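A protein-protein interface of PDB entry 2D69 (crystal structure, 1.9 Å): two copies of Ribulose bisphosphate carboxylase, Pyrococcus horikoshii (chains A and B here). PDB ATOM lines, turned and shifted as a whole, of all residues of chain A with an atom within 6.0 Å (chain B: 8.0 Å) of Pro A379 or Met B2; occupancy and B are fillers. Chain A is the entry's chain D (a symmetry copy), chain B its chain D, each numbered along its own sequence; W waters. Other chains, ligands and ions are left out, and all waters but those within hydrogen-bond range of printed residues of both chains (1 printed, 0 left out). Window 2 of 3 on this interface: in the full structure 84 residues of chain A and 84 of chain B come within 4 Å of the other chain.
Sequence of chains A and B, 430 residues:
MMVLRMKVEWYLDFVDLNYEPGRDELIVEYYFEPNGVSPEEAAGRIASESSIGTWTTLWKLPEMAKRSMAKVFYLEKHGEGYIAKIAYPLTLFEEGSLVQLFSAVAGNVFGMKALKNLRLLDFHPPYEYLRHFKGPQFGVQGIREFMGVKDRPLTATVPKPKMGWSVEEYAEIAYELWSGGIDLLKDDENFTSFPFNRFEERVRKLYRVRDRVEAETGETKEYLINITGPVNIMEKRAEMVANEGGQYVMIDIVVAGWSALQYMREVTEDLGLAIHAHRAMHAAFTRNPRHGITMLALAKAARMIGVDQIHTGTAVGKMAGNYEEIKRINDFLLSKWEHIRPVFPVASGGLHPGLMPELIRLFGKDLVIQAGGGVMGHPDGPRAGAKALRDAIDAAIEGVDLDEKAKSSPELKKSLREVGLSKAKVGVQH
A ring nitrogen (ND1) of His A378 sits at hydrogen-bond distance from the backbone NH (N) of Asp A380 (3.1 Å). The guanidinium group (NH2) of Arg A417 lies within hydrogen-bond range of the backbone carbonyl oxygen (O) of Lys A414 (3.4 Å).
Printed residues of chain B that touch a printed residue of chain A: Met B1, Met B2, Val B3, Leu B4 and Leu B58. Hydrophobic or aromatic side chains of chain B that line the printed part of chain A: Met B1, Val B3, Leu B4 and Leu B58. Along chain B the printed residues that touch a printed residue of chain A span positions 1 to 58. Hydrophobic or aromatic side chains of chain A that line the printed part of chain B: Pro A379.
No position is printed for both chains.
Water W1 lies within hydrogen-bond range of O of His A378 (2.7 Å), N of Leu B58 (2.9 Å) and OG1 of Thr B57 (3.3 Å).
Leu B4 touches Gly A377. His A378 touches Leu B4 (O to CD1, 3.95 Å). Pro A379 touches Met B2. CD1 of Leu B58 touches O of Pro A379, at 3.6 Å. Met B1 touches Arg A417 (CB to NH1, 3.4 Å). OE2 of Glu A418 touches CG1 of Val B3 (3.3 Å).
Of chain B, only Met B2 (3.4 Å) and Leu B58 (3.6 Å) come within 4 Å of Pro A379. Of the printed residues of chain B, Glu A418 touches Val B3. Of the printed residues of chain A, Val B3 touches Glu A418 (3.3 Å). Of the printed residues of chain A, Leu B58 touches Pro A379. Ser A415 touches none of the printed residues of chain B. The nearest residue of chain A that does not touch Met B2 is Arg A417 (4.2 Å).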
ATOM      1  N   GLY A 377     -18.468  27.139 -15.167  1.00  0.00           N
ATOM      2  CA  GLY A 377     -17.908  27.580 -16.429  1.00  0.00           C
ATOM      3  C   GLY A 377     -18.896  27.831 -17.551  1.00  0.00           C
ATOM      4  O   GLY A 377     -18.511  28.345 -18.582  1.00  0.00           O
ATOM      5  N   HIS A 378     -20.160  27.486 -17.370  1.00  0.00           N
ATOM      6  CA  HIS A 378     -21.169  27.743 -18.411  1.00  0.00           C
ATOM      7  C   HIS A 378     -21.096  29.174 -18.975  1.00  0.00           C
ATOM      8  O   HIS A 378     -20.864  30.092 -18.222  1.00  0.00           O
ATOM      9  CB  HIS A 378     -22.559  27.561 -17.812  1.00  0.00           C
ATOM     10  CG  HIS A 378     -23.605  27.270 -18.821  1.00  0.00           C
ATOM     11  ND1 HIS A 378     -24.162  28.248 -19.607  1.00  0.00           N
ATOM     12  CD2 HIS A 378     -24.163  26.104 -19.215  1.00  0.00           C
ATOM     13  CE1 HIS A 378     -25.045  27.705 -20.425  1.00  0.00           C
ATOM     14  NE2 HIS A 378     -25.068  26.403 -20.203  1.00  0.00           N
ATOM     15  N   PRO A 379     -21.294  29.356 -20.274  1.00  0.00           N
ATOM     16  CA  PRO A 379     -21.359  30.685 -20.926  1.00  0.00           C
ATOM     17  C   PRO A 379     -22.381  31.727 -20.462  1.00  0.00           C
ATOM     18  O   PRO A 379     -22.097  32.927 -20.513  1.00  0.00           O
ATOM     19  CB  PRO A 379     -21.743  30.359 -22.364  1.00  0.00           C
ATOM     20  CG  PRO A 379     -21.317  28.982 -22.565  1.00  0.00           C
ATOM     21  CD  PRO A 379     -21.396  28.269 -21.257  1.00  0.00           C
ATOM     22  N   ASP A 380     -23.535  31.268 -19.992  1.00  0.00           N
ATOM     23  CA  ASP A 380     -24.525  32.162 -19.381  1.00  0.00           C
ATOM     24  C   ASP A 380     -24.409  32.170 -17.796  1.00  0.00           C
ATOM     25  O   ASP A 380     -25.270  32.696 -17.114  1.00  0.00           O
ATOM     26  CB  ASP A 380     -25.917  31.738 -19.851  1.00  0.00           C
ATOM     27  CG  ASP A 380     -26.111  31.884 -21.381  1.00  0.00           C
ATOM     28  OD1 ASP A 380     -26.765  30.995 -22.002  1.00  0.00           O
ATOM     29  OD2 ASP A 380     -25.688  32.861 -22.084  1.00  0.00           O
ATOM     30  N   GLY A 381     -23.341  31.626 -17.228  1.00  0.00           N
ATOM     31  CA  GLY A 381     -23.138  31.679 -15.762  1.00  0.00           C
ATOM     32  C   GLY A 381     -23.529  30.429 -15.012  1.00  0.00           C
ATOM     33  O   GLY A 381     -24.086  29.520 -15.609  1.00  0.00           O
ATOM     34  N   LYS A 414     -26.189  24.976 -24.953  1.00  0.00           N
ATOM     35  CA  LYS A 414     -24.945  25.765 -25.034  1.00  0.00           C
ATOM     36  C   LYS A 414     -23.801  24.916 -24.507  1.00  0.00           C
ATOM     37  O   LYS A 414     -22.679  24.919 -25.008  1.00  0.00           O
ATOM     38  CB  LYS A 414     -25.069  27.066 -24.217  1.00  0.00           C
ATOM     39  CG  LYS A 414     -26.134  28.075 -24.738  1.00  0.00           C
ATOM     40  CD  LYS A 414     -25.601  29.520 -24.914  1.00  0.00           C
ATOM     41  CE  LYS A 414     -26.741  30.556 -24.907  1.00  0.00           C
ATOM     42  NZ  LYS A 414     -26.651  31.572 -25.988  1.00  0.00           N
ATOM     43  N   SER A 415     -24.121  24.144 -23.488  1.00  0.00           N
ATOM     44  CA  SER A 415     -23.143  23.294 -22.861  1.00  0.00           C
ATOM     45  C   SER A 415     -22.657  22.204 -23.826  1.00  0.00           C
ATOM     46  O   SER A 415     -21.464  21.884 -23.866  1.00  0.00           O
ATOM     47  CB  SER A 415     -23.743  22.701 -21.580  1.00  0.00           C
ATOM     48  OG  SER A 415     -22.943  21.635 -21.132  1.00  0.00           O
ATOM     49  N   ARG A 417     -22.645  22.227 -27.277  1.00  0.00           N
ATOM     50  CA  ARG A 417     -21.831  22.787 -28.359  1.00  0.00           C
ATOM     51  C   ARG A 417     -20.421  23.046 -27.804  1.00  0.00           C
ATOM     52  O   ARG A 417     -19.421  22.751 -28.479  1.00  0.00           O
ATOM     53  CB  ARG A 417     -22.495  24.048 -28.963  1.00  0.00           C
ATOM     54  CG  ARG A 417     -21.687  24.794 -30.073  1.00  0.00           C
ATOM     55  CD  ARG A 417     -21.036  26.145 -29.621  1.00  0.00           C
ATOM     56  NE  ARG A 417     -21.167  26.449 -28.169  1.00  0.00           N
ATOM     57  CZ  ARG A 417     -21.387  27.673 -27.632  1.00  0.00           C
ATOM     58  NH1 ARG A 417     -21.484  28.764 -28.399  1.00  0.00           N
ATOM     59  NH2 ARG A 417     -21.508  27.810 -26.319  1.00  0.00           N
ATOM     60  N   GLU A 418     -20.347  23.514 -26.550  1.00  0.00           N
ATOM     61  CA  GLU A 418     -19.068  23.859 -25.918  1.00  0.00           C
ATOM     62  C   GLU A 418     -17.967  22.830 -26.237  1.00  0.00           C
ATOM     63  O   GLU A 418     -16.833  23.214 -26.526  1.00  0.00           O
ATOM     64  CB  GLU A 418     -19.213  24.067 -24.396  1.00  0.00           C
ATOM     65  CG  GLU A 418     -18.847  25.470 -23.910  1.00  0.00           C
ATOM     66  CD  GLU A 418     -18.574  25.565 -22.408  1.00  0.00           C
ATOM     67  OE1 GLU A 418     -19.251  24.889 -21.594  1.00  0.00           O
ATOM     68  OE2 GLU A 418     -17.678  26.343 -22.030  1.00  0.00           O
ATOM     69  N   MET B   1     -21.299  31.877 -30.007  1.00  0.00           N
ATOM     70  CA  MET B   1     -21.349  32.420 -28.624  1.00  0.00           C
ATOM     71  C   MET B   1     -20.047  32.122 -27.866  1.00  0.00           C
ATOM     72  O   MET B   1     -19.053  31.761 -28.476  1.00  0.00           O
ATOM     73  CB  MET B   1     -22.598  31.906 -27.898  1.00  0.00           C
ATOM     74  CG  MET B   1     -23.763  31.602 -28.870  1.00  0.00           C
ATOM     75  SD  MET B   1     -24.337  33.057 -29.872  1.00  0.00           S
ATOM     76  CE  MET B   1     -23.347  33.121 -31.525  1.00  0.00           C
ATOM     77  N   MET B   2     -20.066  32.261 -26.545  1.00  0.00           N
ATOM     78  CA  MET B   2     -18.867  32.592 -25.768  1.00  0.00           C
ATOM     79  C   MET B   2     -18.366  31.532 -24.793  1.00  0.00           C
ATOM     80  O   MET B   2     -18.823  31.530 -23.672  1.00  0.00           O
ATOM     81  CB  MET B   2     -19.211  33.834 -24.934  1.00  0.00           C
ATOM     82  CG  MET B   2     -18.170  34.908 -24.916  1.00  0.00           C
ATOM     83  SD  MET B   2     -18.363  36.066 -26.294  1.00  0.00           S
ATOM     84  CE  MET B   2     -20.152  36.747 -26.043  1.00  0.00           C
ATOM     85  N   VAL B   3     -17.417  30.681 -25.178  1.00  0.00           N
ATOM     86  CA  VAL B   3     -16.850  29.648 -24.286  1.00  0.00           C
ATOM     87  C   VAL B   3     -15.778  30.231 -23.337  1.00  0.00           C
ATOM     88  O   VAL B   3     -14.854  30.893 -23.786  1.00  0.00           O
ATOM     89  CB  VAL B   3     -16.234  28.502 -25.112  1.00  0.00           C
ATOM     90  CG1 VAL B   3     -15.554  27.468 -24.245  1.00  0.00           C
ATOM     91  CG2 VAL B   3     -17.309  27.888 -26.042  1.00  0.00           C
ATOM     92  N   LEU B   4     -15.874  29.950 -22.039  1.00  0.00           N
ATOM     93  CA  LEU B   4     -14.962  30.554 -21.087  1.00  0.00           C
ATOM     94  C   LEU B   4     -13.723  29.706 -20.875  1.00  0.00           C
ATOM     95  O   LEU B   4     -13.808  28.505 -20.786  1.00  0.00           O
ATOM     96  CB  LEU B   4     -15.664  30.815 -19.780  1.00  0.00           C
ATOM     97  CG  LEU B   4     -16.895  31.701 -19.828  1.00  0.00           C
ATOM     98  CD1 LEU B   4     -17.362  31.912 -18.434  1.00  0.00           C
ATOM     99  CD2 LEU B   4     -16.618  33.074 -20.475  1.00  0.00           C
ATOM    100  N   ARG B   5     -12.566  30.343 -20.846  1.00  0.00           N
ATOM    101  CA  ARG B   5     -11.288  29.663 -20.668  1.00  0.00           C
ATOM    102  C   ARG B   5     -10.403  30.585 -19.850  1.00  0.00           C
ATOM    103  O   ARG B   5     -10.609  31.792 -19.835  1.00  0.00           O
ATOM    104  CB  ARG B   5     -10.573  29.367 -22.004  1.00  0.00           C
ATOM    105  CG  ARG B   5     -11.448  28.982 -23.209  1.00  0.00           C
ATOM    106  CD  ARG B   5     -11.276  27.526 -23.724  1.00  0.00           C
ATOM    107  NE  ARG B   5     -10.449  27.437 -24.945  1.00  0.00           N
ATOM    108  CZ  ARG B   5      -9.172  27.014 -24.994  1.00  0.00           C
ATOM    109  NH1 ARG B   5      -8.529  26.626 -23.881  1.00  0.00           N
ATOM    110  NH2 ARG B   5      -8.531  26.986 -26.165  1.00  0.00           N
ATOM    111  N   THR B  57     -14.829  31.167 -15.016  1.00  0.00           N
ATOM    112  CA  THR B  57     -16.231  31.468 -14.834  1.00  0.00           C
ATOM    113  C   THR B  57     -16.482  32.918 -15.170  1.00  0.00           C
ATOM    114  O   THR B  57     -15.573  33.743 -15.162  1.00  0.00           O
ATOM    115  CB  THR B  57     -16.693  31.195 -13.351  1.00  0.00           C
ATOM    116  OG1 THR B  57     -18.061  31.587 -13.191  1.00  0.00           O
ATOM    117  CG2 THR B  57     -15.952  32.081 -12.320  1.00  0.00           C
ATOM    118  N   LEU B  58     -17.748  33.212 -15.428  1.00  0.00           N
ATOM    119  CA  LEU B  58     -18.201  34.569 -15.657  1.00  0.00           C
ATOM    120  C   LEU B  58     -18.529  35.227 -14.287  1.00  0.00           C
ATOM    121  O   LEU B  58     -18.542  36.437 -14.136  1.00  0.00           O
ATOM    122  CB  LEU B  58     -19.462  34.499 -16.542  1.00  0.00           C
ATOM    123  CG  LEU B  58     -19.736  35.608 -17.517  1.00  0.00           C
ATOM    124  CD1 LEU B  58     -21.156  35.421 -18.101  1.00  0.00           C
ATOM    125  CD2 LEU B  58     -19.547  36.965 -16.787  1.00  0.00           C
HETATM  126  O   HOH W   1     -19.519  30.988 -16.079  1.00  0.00           O
